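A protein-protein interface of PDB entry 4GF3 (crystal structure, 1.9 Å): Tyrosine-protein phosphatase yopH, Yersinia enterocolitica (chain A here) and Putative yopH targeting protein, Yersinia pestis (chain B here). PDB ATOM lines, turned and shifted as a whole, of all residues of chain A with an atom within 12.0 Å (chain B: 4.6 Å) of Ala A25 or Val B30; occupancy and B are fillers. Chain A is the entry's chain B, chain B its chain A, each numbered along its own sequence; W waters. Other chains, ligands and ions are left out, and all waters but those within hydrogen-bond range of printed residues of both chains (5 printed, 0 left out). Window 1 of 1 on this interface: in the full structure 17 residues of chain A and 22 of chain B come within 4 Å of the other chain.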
ATOM      1  N   GLU A  16      11.799  17.749 -17.779  1.00  0.00           N
ATOM      2  CA  GLU A  16      11.414  17.513 -19.235  1.00  0.00           C
ATOM      3  C   GLU A  16      10.268  18.393 -19.810  1.00  0.00           C
ATOM      4  O   GLU A  16       9.173  18.462 -19.250  1.00  0.00           O
ATOM      5  CB  GLU A  16      11.096  16.021 -19.500  1.00  0.00           C
ATOM      6  CG  GLU A  16      10.546  15.677 -20.908  1.00  0.00           C
ATOM      7  CD  GLU A  16      10.371  14.159 -21.148  1.00  0.00           C
ATOM      8  OE1 GLU A  16       9.211  13.710 -21.450  1.00  0.00           O
ATOM      9  OE2 GLU A  16      11.406  13.415 -21.020  1.00  0.00           O
ATOM     10  N   THR A  17      10.544  19.038 -20.946  1.00  0.00           N
ATOM     11  CA  THR A  17       9.516  19.688 -21.757  1.00  0.00           C
ATOM     12  C   THR A  17       9.675  19.466 -23.285  1.00  0.00           C
ATOM     13  O   THR A  17      10.482  18.649 -23.745  1.00  0.00           O
ATOM     14  CB  THR A  17       9.502  21.206 -21.477  1.00  0.00           C
ATOM     15  OG1 THR A  17      10.801  21.767 -21.744  1.00  0.00           O
ATOM     16  CG2 THR A  17       9.055  21.460 -20.031  1.00  0.00           C
ATOM     17  N   THR A  18       8.872  20.205 -24.041  1.00  0.00           N
ATOM     18  CA  THR A  18       8.863  20.230 -25.496  1.00  0.00           C
ATOM     19  C   THR A  18       9.387  21.600 -25.885  1.00  0.00           C
ATOM     20  O   THR A  18       8.975  22.571 -25.294  1.00  0.00           O
ATOM     21  CB  THR A  18       7.404  19.991 -25.993  1.00  0.00           C
ATOM     22  OG1 THR A  18       7.116  18.595 -25.878  1.00  0.00           O
ATOM     23  CG2 THR A  18       7.205  20.350 -27.424  1.00  0.00           C
ATOM     24  N   PHE A  19      10.314  21.687 -26.841  1.00  0.00           N
ATOM     25  CA  PHE A  19      10.809  22.970 -27.331  1.00  0.00           C
ATOM     26  C   PHE A  19      11.010  22.934 -28.859  1.00  0.00           C
ATOM     27  O   PHE A  19      11.839  22.184 -29.349  1.00  0.00           O
ATOM     28  CB  PHE A  19      12.113  23.348 -26.627  1.00  0.00           C
ATOM     29  CG  PHE A  19      12.678  24.657 -27.098  1.00  0.00           C
ATOM     30  CD1 PHE A  19      12.121  25.858 -26.710  1.00  0.00           C
ATOM     31  CD2 PHE A  19      13.763  24.682 -27.947  1.00  0.00           C
ATOM     32  CE1 PHE A  19      12.633  27.070 -27.174  1.00  0.00           C
ATOM     33  CE2 PHE A  19      14.291  25.888 -28.413  1.00  0.00           C
ATOM     34  CZ  PHE A  19      13.729  27.080 -28.023  1.00  0.00           C
ATOM     35  N   GLN A  20      10.243  23.730 -29.602  1.00  0.00           N
ATOM     36  CA  GLN A  20      10.373  23.761 -31.073  1.00  0.00           C
ATOM     37  C   GLN A  20      10.456  22.334 -31.667  1.00  0.00           C
ATOM     38  O   GLN A  20      11.370  21.986 -32.439  1.00  0.00           O
ATOM     39  CB  GLN A  20      11.607  24.581 -31.444  1.00  0.00           C
ATOM     40  CG  GLN A  20      11.581  25.955 -30.796  1.00  0.00           C
ATOM     41  CD  GLN A  20      12.554  26.953 -31.434  1.00  0.00           C
ATOM     42  OE1 GLN A  20      13.542  26.568 -32.047  1.00  0.00           O
ATOM     43  NE2 GLN A  20      12.262  28.243 -31.287  1.00  0.00           N
ATOM     44  N   GLY A  21       9.537  21.489 -31.231  1.00  0.00           N
ATOM     45  CA  GLY A  21       9.376  20.156 -31.814  1.00  0.00           C
ATOM     46  C   GLY A  21      10.229  19.074 -31.205  1.00  0.00           C
ATOM     47  O   GLY A  21      10.101  17.896 -31.564  1.00  0.00           O
ATOM     48  N   LEU A  22      11.082  19.447 -30.254  1.00  0.00           N
ATOM     49  CA  LEU A  22      11.987  18.528 -29.575  1.00  0.00           C
ATOM     50  C   LEU A  22      11.558  18.284 -28.133  1.00  0.00           C
ATOM     51  O   LEU A  22      11.106  19.204 -27.462  1.00  0.00           O
ATOM     52  CB  LEU A  22      13.386  19.131 -29.502  1.00  0.00           C
ATOM     53  CG  LEU A  22      13.962  19.663 -30.789  1.00  0.00           C
ATOM     54  CD1 LEU A  22      15.336  20.236 -30.475  1.00  0.00           C
ATOM     55  CD2 LEU A  22      14.044  18.582 -31.864  1.00  0.00           C
ATOM     56  N   THR A  23      11.708  17.043 -27.666  1.00  0.00           N
ATOM     57  CA  THR A  23      11.551  16.716 -26.257  1.00  0.00           C
ATOM     58  C   THR A  23      12.924  16.931 -25.639  1.00  0.00           C
ATOM     59  O   THR A  23      13.907  16.451 -26.181  1.00  0.00           O
ATOM     60  CB  THR A  23      11.167  15.236 -26.094  1.00  0.00           C
ATOM     61  OG1 THR A  23       9.891  14.988 -26.685  1.00  0.00           O
ATOM     62  CG2 THR A  23      11.154  14.824 -24.607  1.00  0.00           C
ATOM     63  N   ILE A  24      12.995  17.700 -24.551  1.00  0.00           N
ATOM     64  CA  ILE A  24      14.268  18.071 -23.916  1.00  0.00           C
ATOM     65  C   ILE A  24      14.233  17.934 -22.389  1.00  0.00           C
ATOM     66  O   ILE A  24      13.231  18.234 -21.753  1.00  0.00           O
ATOM     67  CB  ILE A  24      14.707  19.519 -24.275  1.00  0.00           C
ATOM     68  CG1 ILE A  24      13.656  20.525 -23.816  1.00  0.00           C
ATOM     69  CG2 ILE A  24      14.938  19.682 -25.782  1.00  0.00           C
ATOM     70  CD1 ILE A  24      14.149  21.936 -23.970  1.00  0.00           C
ATOM     71  N   ALA A  25      15.330  17.446 -21.800  1.00  0.00           N
ATOM     72  CA  ALA A  25      15.473  17.374 -20.339  1.00  0.00           C
ATOM     73  C   ALA A  25      16.909  17.703 -19.997  1.00  0.00           C
ATOM     74  O   ALA A  25      17.781  17.485 -20.865  1.00  0.00           O
ATOM     75  CB  ALA A  25      15.062  16.004 -19.825  1.00  0.00           C
ATOM     76  N   SER A  26      17.116  18.342 -18.838  1.00  0.00           N
ATOM     77  CA  SER A  26      18.455  18.475 -18.207  1.00  0.00           C
ATOM     78  C   SER A  26      18.980  17.082 -17.911  1.00  0.00           C
ATOM     79  O   SER A  26      18.233  16.198 -17.504  1.00  0.00           O
ATOM     80  CB  SER A  26      18.455  19.292 -16.926  1.00  0.00           C
ATOM     81  OG  SER A  26      19.826  19.527 -16.522  1.00  0.00           O
ATOM     82  N   GLY A  27      20.261  16.884 -18.167  1.00  0.00           N
ATOM     83  CA  GLY A  27      20.891  15.627 -17.881  1.00  0.00           C
ATOM     84  C   GLY A  27      21.321  14.849 -19.093  1.00  0.00           C
ATOM     85  O   GLY A  27      21.050  15.177 -20.243  1.00  0.00           O
ATOM     86  N   ALA A  28      22.022  13.770 -18.811  1.00  0.00           N
ATOM     87  CA  ALA A  28      22.511  12.861 -19.864  1.00  0.00           C
ATOM     88  C   ALA A  28      22.927  11.534 -19.292  1.00  0.00           C
ATOM     89  O   ALA A  28      23.355  11.443 -18.118  1.00  0.00           O
ATOM     90  CB  ALA A  28      23.725  13.467 -20.546  1.00  0.00           C
ATOM     91  N   ARG A  29      22.854  10.500 -20.128  1.00  0.00           N
ATOM     92  CA  ARG A  29      23.445   9.241 -19.779  1.00  0.00           C
ATOM     93  C   ARG A  29      24.960   9.410 -19.496  1.00  0.00           C
ATOM     94  O   ARG A  29      25.673  10.279 -20.111  1.00  0.00           O
ATOM     95  CB  ARG A  29      23.183   8.201 -20.869  1.00  0.00           C
ATOM     96  CG  ARG A  29      23.763   8.532 -22.229  1.00  0.00           C
ATOM     97  CD  ARG A  29      23.217   7.553 -23.281  1.00  0.00           C
ATOM     98  NE  ARG A  29      23.900   7.779 -24.544  1.00  0.00           N
ATOM     99  CZ  ARG A  29      23.420   8.493 -25.563  1.00  0.00           C
ATOM    100  NH1 ARG A  29      22.206   9.040 -25.496  1.00  0.00           N
ATOM    101  NH2 ARG A  29      24.158   8.599 -26.682  1.00  0.00           N
ATOM    102  N   GLU A  30      25.430   8.604 -18.549  1.00  0.00           N
ATOM    103  CA  GLU A  30      26.748   8.792 -17.970  1.00  0.00           C
ATOM    104  C   GLU A  30      27.831   8.672 -19.049  1.00  0.00           C
ATOM    105  O   GLU A  30      28.795   9.434 -19.018  1.00  0.00           O
ATOM    106  CB  GLU A  30      26.991   7.814 -16.820  1.00  0.00           C
ATOM    107  CG  GLU A  30      28.205   8.132 -15.975  1.00  0.00           C
ATOM    108  CD  GLU A  30      28.155   9.532 -15.327  1.00  0.00           C
ATOM    109  OE1 GLU A  30      27.024  10.007 -14.971  1.00  0.00           O
ATOM    110  OE2 GLU A  30      29.273  10.105 -15.153  1.00  0.00           O
ATOM    111  N   SER A  31      27.682   7.740 -19.985  1.00  0.00           N
ATOM    112  CA  SER A  31      28.686   7.540 -21.041  1.00  0.00           C
ATOM    113  C   SER A  31      28.853   8.823 -21.887  1.00  0.00           C
ATOM    114  O   SER A  31      29.929   9.101 -22.376  1.00  0.00           O
ATOM    115  CB  SER A  31      28.334   6.325 -21.901  1.00  0.00           C
ATOM    116  OG  SER A  31      27.062   6.444 -22.480  1.00  0.00           O
ATOM    117  N   GLU A  32      27.767   9.580 -22.065  1.00  0.00           N
ATOM    118  CA  GLU A  32      27.825  10.815 -22.832  1.00  0.00           C
ATOM    119  C   GLU A  32      28.534  11.906 -22.051  1.00  0.00           C
ATOM    120  O   GLU A  32      29.317  12.694 -22.586  1.00  0.00           O
ATOM    121  CB  GLU A  32      26.431  11.315 -23.174  1.00  0.00           C
ATOM    122  CG  GLU A  32      25.996  10.762 -24.454  1.00  0.00           C
ATOM    123  CD  GLU A  32      26.798  11.316 -25.613  1.00  0.00           C
ATOM    124  OE1 GLU A  32      27.166  10.475 -26.450  1.00  0.00           O
ATOM    125  OE2 GLU A  32      27.088  12.580 -25.582  1.00  0.00           O
ATOM    126  N   LYS A  33      28.290  11.919 -20.782  1.00  0.00           N
ATOM    127  CA  LYS A  33      29.074  12.793 -19.905  1.00  0.00           C
ATOM    128  C   LYS A  33      30.560  12.461 -19.874  1.00  0.00           C
ATOM    129  O   LYS A  33      31.401  13.352 -19.733  1.00  0.00           O
ATOM    130  CB  LYS A  33      28.549  12.717 -18.474  1.00  0.00           C
ATOM    131  CG  LYS A  33      27.078  13.098 -18.312  1.00  0.00           C
ATOM    132  CD  LYS A  33      26.850  13.194 -16.808  1.00  0.00           C
ATOM    133  CE  LYS A  33      25.387  13.210 -16.447  1.00  0.00           C
ATOM    134  NZ  LYS A  33      25.251  13.565 -15.051  1.00  0.00           N
ATOM    135  N   VAL A  34      30.858  11.166 -19.933  1.00  0.00           N
ATOM    136  CA  VAL A  34      32.262  10.684 -19.988  1.00  0.00           C
ATOM    137  C   VAL A  34      32.887  11.149 -21.280  1.00  0.00           C
ATOM    138  O   VAL A  34      33.950  11.754 -21.283  1.00  0.00           O
ATOM    139  CB  VAL A  34      32.314   9.178 -19.811  1.00  0.00           C
ATOM    140  CG1 VAL A  34      33.666   8.564 -20.225  1.00  0.00           C
ATOM    141  CG2 VAL A  34      31.972   8.893 -18.365  1.00  0.00           C
ATOM    142  N   PHE A  35      32.162  10.960 -22.364  1.00  0.00           N
ATOM    143  CA  PHE A  35      32.625  11.387 -23.659  1.00  0.00           C
ATOM    144  C   PHE A  35      32.936  12.859 -23.651  1.00  0.00           C
ATOM    145  O   PHE A  35      34.020  13.273 -24.088  1.00  0.00           O
ATOM    146  CB  PHE A  35      31.630  11.000 -24.803  1.00  0.00           C
ATOM    147  CG  PHE A  35      31.612  11.991 -25.933  1.00  0.00           C
ATOM    148  CD1 PHE A  35      32.411  11.829 -27.025  1.00  0.00           C
ATOM    149  CD2 PHE A  35      30.774  13.091 -25.866  1.00  0.00           C
ATOM    150  CE1 PHE A  35      32.392  12.767 -28.051  1.00  0.00           C
ATOM    151  CE2 PHE A  35      30.730  14.023 -26.896  1.00  0.00           C
ATOM    152  CZ  PHE A  35      31.550  13.855 -27.983  1.00  0.00           C
ATOM    153  N   ALA A  36      32.030  13.649 -23.112  1.00  0.00           N
ATOM    154  CA  ALA A  36      32.252  15.106 -23.017  1.00  0.00           C
ATOM    155  C   ALA A  36      33.497  15.464 -22.202  1.00  0.00           C
ATOM    156  O   ALA A  36      34.227  16.378 -22.554  1.00  0.00           O
ATOM    157  CB  ALA A  36      31.037  15.782 -22.389  1.00  0.00           C
ATOM    158  N   LEU A  40      36.590  17.577 -23.566  1.00  0.00           N
ATOM    159  CA  LEU A  40      36.958  18.847 -22.913  1.00  0.00           C
ATOM    160  C   LEU A  40      38.342  18.815 -22.312  1.00  0.00           C
ATOM    161  O   LEU A  40      38.997  19.877 -22.203  1.00  0.00           O
ATOM    162  CB  LEU A  40      35.907  19.208 -21.866  1.00  0.00           C
ATOM    163  CG  LEU A  40      34.628  19.669 -22.527  1.00  0.00           C
ATOM    164  CD1 LEU A  40      33.457  19.544 -21.554  1.00  0.00           C
ATOM    165  CD2 LEU A  40      34.728  21.090 -23.047  1.00  0.00           C
ATOM    166  N   LEU B  15      14.271  27.556 -22.733  1.00  0.00           N
ATOM    167  CA  LEU B  15      13.816  26.228 -23.101  1.00  0.00           C
ATOM    168  C   LEU B  15      12.602  25.739 -22.339  1.00  0.00           C
ATOM    169  O   LEU B  15      11.970  24.772 -22.755  1.00  0.00           O
ATOM    170  CB  LEU B  15      15.004  25.234 -22.899  1.00  0.00           C
ATOM    171  CG  LEU B  15      16.281  25.274 -23.734  1.00  0.00           C
ATOM    172  CD1 LEU B  15      17.280  24.176 -23.268  1.00  0.00           C
ATOM    173  CD2 LEU B  15      15.994  25.186 -25.223  1.00  0.00           C
ATOM    174  N   LEU B  17      12.916  24.623 -19.097  1.00  0.00           N
ATOM    175  CA  LEU B  17      13.393  23.739 -18.008  1.00  0.00           C
ATOM    176  C   LEU B  17      13.586  24.490 -16.711  1.00  0.00           C
ATOM    177  O   LEU B  17      13.878  25.685 -16.732  1.00  0.00           O
ATOM    178  CB  LEU B  17      14.710  23.114 -18.391  1.00  0.00           C
ATOM    179  CG  LEU B  17      14.721  22.346 -19.705  1.00  0.00           C
ATOM    180  CD1 LEU B  17      16.132  21.920 -20.073  1.00  0.00           C
ATOM    181  CD2 LEU B  17      13.787  21.150 -19.574  1.00  0.00           C
ATOM    182  N   ILE B  20      19.483  23.892 -15.600  1.00  0.00           N
ATOM    183  CA  ILE B  20      20.445  23.017 -16.318  1.00  0.00           C
ATOM    184  C   ILE B  20      21.536  22.804 -15.329  1.00  0.00           C
ATOM    185  O   ILE B  20      22.355  23.695 -15.104  1.00  0.00           O
ATOM    186  CB  ILE B  20      20.983  23.661 -17.591  1.00  0.00           C
ATOM    187  CG1 ILE B  20      19.802  23.709 -18.558  1.00  0.00           C
ATOM    188  CG2 ILE B  20      22.122  22.797 -18.189  1.00  0.00           C
ATOM    189  CD1 ILE B  20      20.181  24.198 -19.894  1.00  0.00           C
ATOM    190  N   ALA B  29      24.349  19.412 -19.472  1.00  0.00           N
ATOM    191  CA  ALA B  29      23.850  18.701 -20.651  1.00  0.00           C
ATOM    192  C   ALA B  29      22.311  18.746 -20.746  1.00  0.00           C
ATOM    193  O   ALA B  29      21.616  18.743 -19.732  1.00  0.00           O
ATOM    194  CB  ALA B  29      24.360  17.225 -20.654  1.00  0.00           C
ATOM    195  N   VAL B  30      21.836  18.697 -21.990  1.00  0.00           N
ATOM    196  CA  VAL B  30      20.480  18.551 -22.295  1.00  0.00           C
ATOM    197  C   VAL B  30      20.380  17.306 -23.183  1.00  0.00           C
ATOM    198  O   VAL B  30      21.109  17.209 -24.192  1.00  0.00           O
ATOM    199  CB  VAL B  30      19.988  19.831 -23.015  1.00  0.00           C
ATOM    200  CG1 VAL B  30      18.554  19.657 -23.477  1.00  0.00           C
ATOM    201  CG2 VAL B  30      20.012  20.986 -22.016  1.00  0.00           C
ATOM    202  N   THR B  31      19.413  16.422 -22.865  1.00  0.00           N
ATOM    203  CA  THR B  31      19.058  15.292 -23.684  1.00  0.00           C
ATOM    204  C   THR B  31      17.865  15.640 -24.572  1.00  0.00           C
ATOM    205  O   THR B  31      16.825  16.140 -24.083  1.00  0.00           O
ATOM    206  CB  THR B  31      18.786  14.041 -22.816  1.00  0.00           C
ATOM    207  OG1 THR B  31      20.029  13.647 -22.190  1.00  0.00           O
ATOM    208  CG2 THR B  31      18.271  12.884 -23.646  1.00  0.00           C
ATOM    209  N   ILE B  32      18.037  15.341 -25.855  1.00  0.00           N
ATOM    210  CA  ILE B  32      17.097  15.682 -26.891  1.00  0.00           C
ATOM    211  C   ILE B  32      16.514  14.436 -27.566  1.00  0.00           C
ATOM    212  O   ILE B  32      17.237  13.616 -28.158  1.00  0.00           O
ATOM    213  CB  ILE B  32      17.712  16.613 -27.936  1.00  0.00           C
ATOM    214  CG1 ILE B  32      18.142  17.931 -27.282  1.00  0.00           C
ATOM    215  CG2 ILE B  32      16.697  16.839 -29.058  1.00  0.00           C
ATOM    216  CD1 ILE B  32      19.574  18.238 -27.478  1.00  0.00           C
ATOM    217  N   TRP B  36      19.872  12.269 -28.318  1.00  0.00           N
ATOM    218  CA  TRP B  36      20.939  13.168 -28.553  1.00  0.00           C
ATOM    219  C   TRP B  36      21.257  13.951 -27.272  1.00  0.00           C
ATOM    220  O   TRP B  36      20.375  14.330 -26.504  1.00  0.00           O
ATOM    221  CB  TRP B  36      20.587  14.248 -29.574  1.00  0.00           C
ATOM    222  CG  TRP B  36      20.204  13.856 -30.978  1.00  0.00           C
ATOM    223  CD1 TRP B  36      19.055  14.250 -31.626  1.00  0.00           C
ATOM    224  CD2 TRP B  36      20.992  13.164 -31.953  1.00  0.00           C
ATOM    225  NE1 TRP B  36      19.068  13.808 -32.920  1.00  0.00           N
ATOM    226  CE2 TRP B  36      20.233  13.129 -33.149  1.00  0.00           C
ATOM    227  CE3 TRP B  36      22.226  12.530 -31.923  1.00  0.00           C
ATOM    228  CZ2 TRP B  36      20.676  12.494 -34.309  1.00  0.00           C
ATOM    229  CZ3 TRP B  36      22.662  11.888 -33.066  1.00  0.00           C
ATOM    230  CH2 TRP B  36      21.876  11.864 -34.246  1.00  0.00           C
ATOM    231  N   VAL B  37      22.511  14.329 -27.142  1.00  0.00           N
ATOM    232  CA  VAL B  37      22.937  15.109 -25.982  1.00  0.00           C
ATOM    233  C   VAL B  37      23.779  16.283 -26.421  1.00  0.00           C
ATOM    234  O   VAL B  37      24.808  16.127 -27.079  1.00  0.00           O
ATOM    235  CB  VAL B  37      23.721  14.204 -24.959  1.00  0.00           C
ATOM    236  CG1 VAL B  37      24.164  15.039 -23.792  1.00  0.00           C
ATOM    237  CG2 VAL B  37      22.869  13.068 -24.478  1.00  0.00           C
ATOM    238  N   VAL B  38      23.347  17.496 -26.044  1.00  0.00           N
ATOM    239  CA  VAL B  38      24.092  18.666 -26.271  1.00  0.00           C
ATOM    240  C   VAL B  38      24.721  18.996 -24.938  1.00  0.00           C
ATOM    241  O   VAL B  38      24.065  19.170 -23.923  1.00  0.00           O
ATOM    242  CB  VAL B  38      23.224  19.851 -26.761  1.00  0.00           C
ATOM    243  CG1 VAL B  38      23.996  21.134 -26.717  1.00  0.00           C
ATOM    244  CG2 VAL B  38      22.780  19.664 -28.225  1.00  0.00           C
ATOM    245  N   LEU B 109      21.429  25.230 -29.959  1.00  0.00           N
ATOM    246  CA  LEU B 109      20.995  23.879 -29.640  1.00  0.00           C
ATOM    247  C   LEU B 109      20.175  23.265 -30.802  1.00  0.00           C
ATOM    248  O   LEU B 109      20.377  22.112 -31.254  1.00  0.00           O
ATOM    249  CB  LEU B 109      20.224  23.900 -28.329  1.00  0.00           C
ATOM    250  CG  LEU B 109      19.749  22.499 -27.878  1.00  0.00           C
ATOM    251  CD1 LEU B 109      19.746  22.376 -26.364  1.00  0.00           C
ATOM    252  CD2 LEU B 109      18.381  22.182 -28.428  1.00  0.00           C
HETATM  253  O   HOH W   1      22.860  19.248 -16.946  1.00  0.00           O
HETATM  254  O   HOH W   2       9.550  24.756 -23.685  1.00  0.00           O
HETATM  255  O   HOH W   3      26.658  14.231 -27.623  1.00  0.00           O
HETATM  256  O   HOH W   4      14.898  13.994 -24.497  1.00  0.00           O
HETATM  257  O   HOH W   5      21.177  11.024 -22.438  1.00  0.00           O
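Water W2 bridges O of Leu B15 (2.6 Å) and O of Thr A18 (2.8 Å).
Water W3 lies within hydrogen-bond range of OE2 of Glu A32 (2.7 Å) and O of Val B37 (2.7 Å).
Water W5 lies within hydrogen-bond range of OG1 of Thr B31 (2.9 Å) and N of Arg A29 (2.9 Å).
Water W4 lies within hydrogen-bond range of the backbone carbonyl oxygen (O) of Thr B31 (2.9 Å) and the backbone carbonyl oxygen (O) of Thr A23 (3.1 Å).
Water W1 bridges N of Ala B29 and OG of Ser A26.
The backbone carbonyl oxygen (O) of Val B30 sits at hydrogen-bond distance from the backbone NH (N) of Val B38, 2.9 Å away.
The backbone NH of Ile A24 is in hydrogen-bond range of the backbone carbonyl oxygen of Thr A17 (2.8 Å).
NH2 of Arg A29 is in salt-bridge range of OE1 of Glu A32 (3.6 Å).
Printed residues of chain B within 4 Å of Phe A19: Leu B15.
Printed residues of chain B within 4 Å of Ile A24: Leu B15 (3.6 Å), Leu B17 (3.7 Å), Val B30 (3.9 Å), Thr B31 (3.2 Å) and Ile B32 (3.9 Å).
Ala A25 touches just these residues of chain B: Val B30 and Thr B31.
Of the printed residues of chain B, Ser A26 touches Leu B17 (3.9 Å), Ile B20 (3.6 Å) and Ala B29 (3.5 Å).
Ile B20 touches just one residue of chain A: Ser A26 (3.6 Å).
Of the printed residues of chain A, Ala B29 touches Ser A26, Gly A27 and Ala A28.
Thr B31 touches just these residues of chain A: Thr A23, Ile A24, Ala A25, Gly A27 and Ala A28.
Ile B32 touches just these residues of chain A: Leu A22 (3.9 Å), Thr A23 (3.4 Å) and Ile A24 (3.9 Å).
Trp B36 touches none of the printed residues of chain A.
No residue of chain A comes within 4 Å of Val B38.
OG1 of Thr A17 is in hydrogen-bond range of O of Leu B15.
The backbone carbonyl oxygen (O) of Ala B29 sits at hydrogen-bond distance from the backbone NH (N) of Gly A27 (2.8 Å).
N of Thr B31 is in hydrogen-bond range of O of Ala A25, 2.8 Å away.
OG1 of Thr B31 sits at hydrogen-bond distance from O of Gly A27 (2.7 Å).
Of the 22 printed residues of chain A, 10 touch a printed residue of chain B.
Printed residues of chain A that touch a printed residue of chain B: Thr A17, Phe A19, Leu A22, Thr A23, Ile A24, Ala A25, Ser A26, Gly A27, Ala A28 and Glu A32.
Of the 11 printed residues of chain B, 8 touch a printed residue of chain A.
Hydrophobic or aromatic side chains of chain B that line the printed part of chain A: Leu B15, Leu B17, Ala B29, Val B30, Ile B32 and Val B37.
Among the printed residues, 23 pairs touch across the chains.
Phe A19 touches Leu B15.
Ile B32 touches Thr A23.
Ile A24 touches Leu B15 (CD1 to CB, 3.6 Å).
CB of Ile A24 touches CG1 of Val B30 (3.9 Å).
Ile A24 touches Thr B31.
Ile A24 touches Ile B32 (CG2 to CG1, 3.9 Å).
Leu B17 touches Ser A26 (CD1 to N, 3.9 Å).
Ile B20 touches Ser A26 (CA to OG, 3.6 Å).
C of Val B30 touches O of Gly A27, 3.7 Å away.
OE2 of Glu A32 touches CB of Val B37, at 3.8 Å.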
